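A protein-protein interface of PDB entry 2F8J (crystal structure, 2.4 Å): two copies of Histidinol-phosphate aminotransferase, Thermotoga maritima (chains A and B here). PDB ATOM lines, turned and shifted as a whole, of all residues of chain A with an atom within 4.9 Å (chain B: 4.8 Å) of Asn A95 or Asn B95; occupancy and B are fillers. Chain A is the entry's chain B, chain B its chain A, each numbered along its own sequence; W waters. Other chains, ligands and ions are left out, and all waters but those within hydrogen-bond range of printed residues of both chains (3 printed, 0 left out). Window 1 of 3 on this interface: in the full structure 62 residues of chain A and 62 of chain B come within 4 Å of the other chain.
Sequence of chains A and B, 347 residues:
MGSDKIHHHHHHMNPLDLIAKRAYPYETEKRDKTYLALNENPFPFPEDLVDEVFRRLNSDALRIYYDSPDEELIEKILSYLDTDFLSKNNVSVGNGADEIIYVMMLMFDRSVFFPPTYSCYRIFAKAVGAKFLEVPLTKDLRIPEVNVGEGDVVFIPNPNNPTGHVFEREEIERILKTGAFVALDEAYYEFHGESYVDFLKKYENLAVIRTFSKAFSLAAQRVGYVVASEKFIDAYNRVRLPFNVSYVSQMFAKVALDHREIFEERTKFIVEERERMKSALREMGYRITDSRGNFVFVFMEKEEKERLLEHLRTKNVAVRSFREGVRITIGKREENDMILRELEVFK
Asn A95 touches Asn B244, and with the chains exchanged Asn A244 touches Asn B95.
Asp A98 touches Leu B241, and with the chains exchanged Leu A241 touches Asp B98.
Glu A99 touches Leu B241, and with the chains exchanged Leu A241 touches Glu B99.
Arg A222 touches Phe B243, and with the chains exchanged Phe A243 touches Arg B222.
Positions printed for both chains: 93, 94, 95, 96, 97, 98, 99, 222, 241, 243, 244 and 245.
Of the 9 pairs that touch across the chains among the printed residues, 9 have their exchanged pair printed and touching as well.
Asn A95 touches just these residues of chain B: Asn B95 and Asn B244.
Of the printed residues of chain B, Glu A99 touches Leu B241.
Printed residues of chain B within 4 Å of Leu A241: Asp B98 (3.97 Å) and Glu B99 (3.7 Å).
Val A245 touches none of the printed residues of chain B.
Asn B95 touches two residues of chain A.
Gly B96 touches none of the printed residues of chain A.
Of the printed residues of chain A, Arg B222 touches Phe A243 (3.0 Å).
The nearest residue of chain B that does not touch Asn A95 is Phe B243 (4.3 Å).
Of the 12 printed residues of chain B, 7 touch a printed residue of chain A.
Printed residues of chain B that touch a printed residue of chain A: Asn B95, Asp B98, Glu B99, Arg B222, Leu B241, Phe B243 and Asn B244.
Printed residues of chain A that touch a printed residue of chain B: Asn A95, Asp A98, Glu A99, Arg A222, Leu A241, Phe A243 and Asn A244.
Hydrophobic or aromatic side chains of chain A within 4 Å of the printed part of chain B: Leu A241 and Phe A243.
Among the printed residues, 9 pairs touch across the chains.
Among the printed residues, no Asp or Glu carboxylate lies within 4 Å of a Lys or Arg side-chain nitrogen of the other chain.
The guanidinium group of Arg B222 is in hydrogen-bond range of the backbone carbonyl oxygen of Phe A243 (3.0 Å).
The guanidinium group (NE) of Arg A222 sits at hydrogen-bond distance from the backbone carbonyl oxygen (O) of Phe B243 (2.9 Å).
The backbone carbonyl oxygen (O) of Asn B244 is in hydrogen-bond range of the side-chain amide nitrogen (ND2) of Asn A95.
ND2 of Asn B95 is in hydrogen-bond range of O of Asn A244 (2.9 Å).
Among the printed residues, pairs that only touch across the chains: Asn A95 with Asn B95, Glu A99 with Leu B241, Leu A241 with Glu B99, Asp A98 with Leu B241 and Leu A241 with Asp B98.
Water W2 lies within hydrogen-bond range of O of Phe B243 (2.7 Å), O of Asn A95 (2.7 Å) and NH2 of Arg A222 (3.1 Å).
Water W3 lies within hydrogen-bond range of OD2 of Asp A98 (2.8 Å) and N of Phe B243 (3.0 Å).
Water W1 lies within hydrogen-bond range of the side-chain carboxylate of Asp B98 and the backbone NH of Phe A243.
The side-chain carboxylate of Glu B99 sits at hydrogen-bond distance from the backbone NH of Asn B95 (2.7 Å).
The backbone NH of Gly B96 lies within hydrogen-bond range of the backbone carbonyl oxygen of Arg B222.
The guanidinium group of Arg A222 lies within salt-bridge range of the side-chain carboxylate of Asp A98 (3.9 Å).
OE1 of Glu B99 lies within hydrogen-bond range of ND2 of Asn B244 (2.7 Å).
The backbone carbonyl oxygen (O) of Val B93 is in hydrogen-bond range of the side-chain amide nitrogen (ND2) of Asn B244.
N of Gly A96 is in hydrogen-bond range of O of Arg A222 (3.2 Å).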
ATOM      1  N   VAL A  93     -14.686  -7.056  26.219  1.00  0.00           N
ATOM      2  CA  VAL A  93     -13.508  -7.909  25.974  1.00  0.00           C
ATOM      3  C   VAL A  93     -12.629  -7.393  24.858  1.00  0.00           C
ATOM      4  O   VAL A  93     -13.067  -6.594  24.007  1.00  0.00           O
ATOM      5  CB  VAL A  93     -13.859  -9.389  25.641  1.00  0.00           C
ATOM      6  CG1 VAL A  93     -14.520 -10.095  26.838  1.00  0.00           C
ATOM      7  CG2 VAL A  93     -14.715  -9.509  24.380  1.00  0.00           C
ATOM      8  N   GLY A  94     -11.399  -7.900  24.851  1.00  0.00           N
ATOM      9  CA  GLY A  94     -10.458  -7.637  23.785  1.00  0.00           C
ATOM     10  C   GLY A  94      -9.661  -8.857  23.363  1.00  0.00           C
ATOM     11  O   GLY A  94      -9.537  -9.834  24.112  1.00  0.00           O
ATOM     12  N   ASN A  95      -9.127  -8.779  22.144  1.00  0.00           N
ATOM     13  CA  ASN A  95      -8.188  -9.733  21.614  1.00  0.00           C
ATOM     14  C   ASN A  95      -6.866  -9.512  22.361  1.00  0.00           C
ATOM     15  O   ASN A  95      -5.933  -8.883  21.858  1.00  0.00           O
ATOM     16  CB  ASN A  95      -8.036  -9.521  20.085  1.00  0.00           C
ATOM     17  CG  ASN A  95      -7.232 -10.615  19.407  1.00  0.00           C
ATOM     18  OD1 ASN A  95      -7.106 -11.704  19.916  1.00  0.00           O
ATOM     19  ND2 ASN A  95      -6.691 -10.320  18.245  1.00  0.00           N
ATOM     20  N   GLY A  96      -6.810 -10.020  23.582  1.00  0.00           N
ATOM     21  CA  GLY A  96      -5.762  -9.685  24.507  1.00  0.00           C
ATOM     22  C   GLY A  96      -6.013  -8.329  25.140  1.00  0.00           C
ATOM     23  O   GLY A  96      -6.768  -7.502  24.624  1.00  0.00           O
ATOM     24  N   ALA A  97      -5.392  -8.100  26.290  1.00  0.00           N
ATOM     25  CA  ALA A  97      -5.296  -6.749  26.846  1.00  0.00           C
ATOM     26  C   ALA A  97      -4.615  -5.771  25.867  1.00  0.00           C
ATOM     27  O   ALA A  97      -4.869  -4.571  25.898  1.00  0.00           O
ATOM     28  CB  ALA A  97      -4.530  -6.785  28.151  1.00  0.00           C
ATOM     29  N   ASP A  98      -3.724  -6.290  25.030  1.00  0.00           N
ATOM     30  CA  ASP A  98      -3.100  -5.490  23.998  1.00  0.00           C
ATOM     31  C   ASP A  98      -4.130  -4.759  23.141  1.00  0.00           C
ATOM     32  O   ASP A  98      -3.980  -3.568  22.891  1.00  0.00           O
ATOM     33  CB  ASP A  98      -2.229  -6.356  23.117  1.00  0.00           C
ATOM     34  CG  ASP A  98      -0.841  -6.638  23.723  1.00  0.00           C
ATOM     35  OD1 ASP A  98      -0.479  -6.097  24.816  1.00  0.00           O
ATOM     36  OD2 ASP A  98      -0.102  -7.414  23.055  1.00  0.00           O
ATOM     37  N   GLU A  99      -5.193  -5.457  22.721  1.00  0.00           N
ATOM     38  CA  GLU A  99      -6.208  -4.850  21.854  1.00  0.00           C
ATOM     39  C   GLU A  99      -6.906  -3.716  22.566  1.00  0.00           C
ATOM     40  O   GLU A  99      -7.230  -2.707  21.969  1.00  0.00           O
ATOM     41  CB  GLU A  99      -7.236  -5.882  21.372  1.00  0.00           C
ATOM     42  CG  GLU A  99      -8.053  -5.382  20.147  1.00  0.00           C
ATOM     43  CD  GLU A  99      -9.378  -6.125  19.879  1.00  0.00           C
ATOM     44  OE1 GLU A  99     -10.042  -6.579  20.840  1.00  0.00           O
ATOM     45  OE2 GLU A  99      -9.757  -6.243  18.685  1.00  0.00           O
ATOM     46  N   ARG A 222      -5.495 -15.257  23.748  1.00  0.00           N
ATOM     47  CA  ARG A 222      -5.760 -13.807  23.633  1.00  0.00           C
ATOM     48  C   ARG A 222      -7.124 -13.361  24.157  1.00  0.00           C
ATOM     49  O   ARG A 222      -7.984 -12.963  23.362  1.00  0.00           O
ATOM     50  CB  ARG A 222      -5.656 -13.320  22.157  1.00  0.00           C
ATOM     51  CG  ARG A 222      -4.635 -13.997  21.241  1.00  0.00           C
ATOM     52  CD  ARG A 222      -3.232 -13.867  21.749  1.00  0.00           C
ATOM     53  NE  ARG A 222      -2.914 -12.470  21.996  1.00  0.00           N
ATOM     54  CZ  ARG A 222      -2.645 -11.926  23.174  1.00  0.00           C
ATOM     55  NH1 ARG A 222      -2.605 -12.666  24.272  1.00  0.00           N
ATOM     56  NH2 ARG A 222      -2.402 -10.618  23.246  1.00  0.00           N
ATOM     57  N   LEU A 241     -13.135  -3.754  16.804  1.00  0.00           N
ATOM     58  CA  LEU A 241     -13.700  -4.763  15.902  1.00  0.00           C
ATOM     59  C   LEU A 241     -14.834  -5.504  16.612  1.00  0.00           C
ATOM     60  O   LEU A 241     -14.672  -5.899  17.754  1.00  0.00           O
ATOM     61  CB  LEU A 241     -12.631  -5.777  15.500  1.00  0.00           C
ATOM     62  CG  LEU A 241     -11.563  -5.262  14.557  1.00  0.00           C
ATOM     63  CD1 LEU A 241     -10.423  -6.233  14.490  1.00  0.00           C
ATOM     64  CD2 LEU A 241     -12.162  -4.998  13.194  1.00  0.00           C
ATOM     65  N   PHE A 243     -16.212  -8.541  16.038  1.00  0.00           N
ATOM     66  CA  PHE A 243     -15.981  -9.952  16.295  1.00  0.00           C
ATOM     67  C   PHE A 243     -14.492 -10.177  16.590  1.00  0.00           C
ATOM     68  O   PHE A 243     -13.751 -10.730  15.794  1.00  0.00           O
ATOM     69  CB  PHE A 243     -16.485 -10.773  15.095  1.00  0.00           C
ATOM     70  CG  PHE A 243     -17.935 -10.519  14.757  1.00  0.00           C
ATOM     71  CD1 PHE A 243     -18.936 -11.045  15.547  1.00  0.00           C
ATOM     72  CD2 PHE A 243     -18.289  -9.729  13.666  1.00  0.00           C
ATOM     73  CE1 PHE A 243     -20.269 -10.804  15.254  1.00  0.00           C
ATOM     74  CE2 PHE A 243     -19.621  -9.489  13.370  1.00  0.00           C
ATOM     75  CZ  PHE A 243     -20.608 -10.036  14.166  1.00  0.00           C
ATOM     76  N   ASN A 244     -14.058  -9.715  17.755  1.00  0.00           N
ATOM     77  CA  ASN A 244     -12.643  -9.605  18.056  1.00  0.00           C
ATOM     78  C   ASN A 244     -12.058 -10.799  18.837  1.00  0.00           C
ATOM     79  O   ASN A 244     -10.845 -11.011  18.844  1.00  0.00           O
ATOM     80  CB  ASN A 244     -12.361  -8.266  18.777  1.00  0.00           C
ATOM     81  CG  ASN A 244     -13.125  -8.103  20.103  1.00  0.00           C
ATOM     82  OD1 ASN A 244     -14.203  -8.639  20.281  1.00  0.00           O
ATOM     83  ND2 ASN A 244     -12.571  -7.332  21.005  1.00  0.00           N
ATOM     84  N   VAL A 245     -12.911 -11.568  19.492  1.00  0.00           N
ATOM     85  CA  VAL A 245     -12.483 -12.741  20.271  1.00  0.00           C
ATOM     86  C   VAL A 245     -13.254 -13.912  19.739  1.00  0.00           C
ATOM     87  O   VAL A 245     -14.492 -13.856  19.661  1.00  0.00           O
ATOM     88  CB  VAL A 245     -12.754 -12.588  21.806  1.00  0.00           C
ATOM     89  CG1 VAL A 245     -12.208 -13.769  22.575  1.00  0.00           C
ATOM     90  CG2 VAL A 245     -12.131 -11.295  22.326  1.00  0.00           C
ATOM     91  N   VAL B  93      -1.149 -12.223   8.362  1.00  0.00           N
ATOM     92  CA  VAL B  93      -2.501 -12.589   8.835  1.00  0.00           C
ATOM     93  C   VAL B  93      -3.206 -11.469   9.598  1.00  0.00           C
ATOM     94  O   VAL B  93      -2.596 -10.511  10.067  1.00  0.00           O
ATOM     95  CB  VAL B  93      -2.507 -13.865   9.741  1.00  0.00           C
ATOM     96  CG1 VAL B  93      -1.980 -15.077   8.982  1.00  0.00           C
ATOM     97  CG2 VAL B  93      -1.706 -13.627  11.048  1.00  0.00           C
ATOM     98  N   GLY B  94      -4.522 -11.629   9.705  1.00  0.00           N
ATOM     99  CA  GLY B  94      -5.369 -10.753  10.490  1.00  0.00           C
ATOM    100  C   GLY B  94      -6.405 -11.519  11.288  1.00  0.00           C
ATOM    101  O   GLY B  94      -6.738 -12.663  10.972  1.00  0.00           O
ATOM    102  N   ASN B  95      -6.869 -10.879  12.352  1.00  0.00           N
ATOM    103  CA  ASN B  95      -7.991 -11.350  13.142  1.00  0.00           C
ATOM    104  C   ASN B  95      -9.269 -11.081  12.333  1.00  0.00           C
ATOM    105  O   ASN B  95      -9.964 -10.102  12.558  1.00  0.00           O
ATOM    106  CB  ASN B  95      -8.026 -10.644  14.513  1.00  0.00           C
ATOM    107  CG  ASN B  95      -9.088 -11.205  15.415  1.00  0.00           C
ATOM    108  OD1 ASN B  95      -9.423 -12.366  15.298  1.00  0.00           O
ATOM    109  ND2 ASN B  95      -9.621 -10.392  16.325  1.00  0.00           N
ATOM    110  N   GLY B  96      -9.520 -11.950  11.362  1.00  0.00           N
ATOM    111  CA  GLY B  96     -10.476 -11.690  10.309  1.00  0.00           C
ATOM    112  C   GLY B  96      -9.860 -10.794   9.236  1.00  0.00           C
ATOM    113  O   GLY B  96      -8.881 -10.090   9.479  1.00  0.00           O
ATOM    114  N   ALA B  97     -10.430 -10.837   8.040  1.00  0.00           N
ATOM    115  CA  ALA B  97     -10.152  -9.832   7.025  1.00  0.00           C
ATOM    116  C   ALA B  97     -10.525  -8.437   7.519  1.00  0.00           C
ATOM    117  O   ALA B  97      -9.932  -7.436   7.104  1.00  0.00           O
ATOM    118  CB  ALA B  97     -10.879 -10.160   5.762  1.00  0.00           C
ATOM    119  N   ASP B  98     -11.510  -8.375   8.407  1.00  0.00           N
ATOM    120  CA  ASP B  98     -11.924  -7.131   9.037  1.00  0.00           C
ATOM    121  C   ASP B  98     -10.756  -6.395   9.689  1.00  0.00           C
ATOM    122  O   ASP B  98     -10.656  -5.173   9.524  1.00  0.00           O
ATOM    123  CB  ASP B  98     -13.012  -7.395  10.089  1.00  0.00           C
ATOM    124  CG  ASP B  98     -14.459  -7.382   9.504  1.00  0.00           C
ATOM    125  OD1 ASP B  98     -14.637  -7.264   8.270  1.00  0.00           O
ATOM    126  OD2 ASP B  98     -15.420  -7.500  10.307  1.00  0.00           O
ATOM    127  N   GLU B  99      -9.883  -7.116  10.413  1.00  0.00           N
ATOM    128  CA  GLU B  99      -8.722  -6.481  11.033  1.00  0.00           C
ATOM    129  C   GLU B  99      -7.759  -5.922   9.996  1.00  0.00           C
ATOM    130  O   GLU B  99      -7.116  -4.901  10.222  1.00  0.00           O
ATOM    131  CB  GLU B  99      -7.960  -7.446  11.948  1.00  0.00           C
ATOM    132  CG  GLU B  99      -6.898  -6.736  12.809  1.00  0.00           C
ATOM    133  CD  GLU B  99      -5.945  -7.677  13.558  1.00  0.00           C
ATOM    134  OE1 GLU B  99      -5.438  -8.648  12.954  1.00  0.00           O
ATOM    135  OE2 GLU B  99      -5.681  -7.422  14.756  1.00  0.00           O
ATOM    136  N   ARG B 222     -12.048 -16.393  12.936  1.00  0.00           N
ATOM    137  CA  ARG B 222     -11.432 -15.122  12.545  1.00  0.00           C
ATOM    138  C   ARG B 222      -9.999 -15.272  12.007  1.00  0.00           C
ATOM    139  O   ARG B 222      -9.044 -14.848  12.645  1.00  0.00           O
ATOM    140  CB  ARG B 222     -11.379 -14.135  13.735  1.00  0.00           C
ATOM    141  CG  ARG B 222     -12.520 -14.154  14.783  1.00  0.00           C
ATOM    142  CD  ARG B 222     -13.857 -13.855  14.196  1.00  0.00           C
ATOM    143  NE  ARG B 222     -13.860 -12.594  13.452  1.00  0.00           N
ATOM    144  CZ  ARG B 222     -14.045 -12.474  12.146  1.00  0.00           C
ATOM    145  NH1 ARG B 222     -14.250 -13.549  11.386  1.00  0.00           N
ATOM    146  NH2 ARG B 222     -14.021 -11.257  11.607  1.00  0.00           N
ATOM    147  N   LEU B 241      -1.557  -5.501  15.741  1.00  0.00           N
ATOM    148  CA  LEU B 241      -1.266  -6.195  16.978  1.00  0.00           C
ATOM    149  C   LEU B 241      -0.345  -7.375  16.703  1.00  0.00           C
ATOM    150  O   LEU B 241      -0.570  -8.146  15.767  1.00  0.00           O
ATOM    151  CB  LEU B 241      -2.567  -6.652  17.648  1.00  0.00           C
ATOM    152  CG  LEU B 241      -3.409  -5.538  18.280  1.00  0.00           C
ATOM    153  CD1 LEU B 241      -4.778  -6.097  18.634  1.00  0.00           C
ATOM    154  CD2 LEU B 241      -2.705  -4.955  19.524  1.00  0.00           C
ATOM    155  N   PHE B 243       0.212 -10.186  18.436  1.00  0.00           N
ATOM    156  CA  PHE B 243      -0.379 -11.511  18.702  1.00  0.00           C
ATOM    157  C   PHE B 243      -1.866 -11.465  18.415  1.00  0.00           C
ATOM    158  O   PHE B 243      -2.665 -11.455  19.316  1.00  0.00           O
ATOM    159  CB  PHE B 243      -0.076 -11.931  20.142  1.00  0.00           C
ATOM    160  CG  PHE B 243       1.397 -11.936  20.458  1.00  0.00           C
ATOM    161  CD1 PHE B 243       2.215 -12.945  19.965  1.00  0.00           C
ATOM    162  CD2 PHE B 243       1.964 -10.925  21.227  1.00  0.00           C
ATOM    163  CE1 PHE B 243       3.586 -12.950  20.239  1.00  0.00           C
ATOM    164  CE2 PHE B 243       3.335 -10.919  21.519  1.00  0.00           C
ATOM    165  CZ  PHE B 243       4.148 -11.927  21.024  1.00  0.00           C
ATOM    166  N   ASN B 244      -2.204 -11.387  17.132  1.00  0.00           N
ATOM    167  CA  ASN B 244      -3.542 -11.008  16.693  1.00  0.00           C
ATOM    168  C   ASN B 244      -4.444 -12.198  16.338  1.00  0.00           C
ATOM    169  O   ASN B 244      -5.669 -12.067  16.323  1.00  0.00           O
ATOM    170  CB  ASN B 244      -3.475  -9.968  15.541  1.00  0.00           C
ATOM    171  CG  ASN B 244      -2.738 -10.477  14.300  1.00  0.00           C
ATOM    172  OD1 ASN B 244      -1.870 -11.338  14.368  1.00  0.00           O
ATOM    173  ND2 ASN B 244      -3.087  -9.921  13.155  1.00  0.00           N
ATOM    174  N   VAL B 245      -3.838 -13.350  16.078  1.00  0.00           N
ATOM    175  CA  VAL B 245      -4.579 -14.570  15.749  1.00  0.00           C
ATOM    176  C   VAL B 245      -4.102 -15.657  16.698  1.00  0.00           C
ATOM    177  O   VAL B 245      -2.900 -15.887  16.819  1.00  0.00           O
ATOM    178  CB  VAL B 245      -4.322 -15.045  14.279  1.00  0.00           C
ATOM    179  CG1 VAL B 245      -5.145 -16.297  13.964  1.00  0.00           C
ATOM    180  CG2 VAL B 245      -4.624 -13.948  13.282  1.00  0.00           C
HETATM  181  O   HOH W   1     -14.785  -7.826  13.182  1.00  0.00           O
HETATM  182  O   HOH W   2      -3.509  -9.335  20.670  1.00  0.00           O
HETATM  183  O   HOH W   3      -0.903  -8.402  20.537  1.00  0.00           O
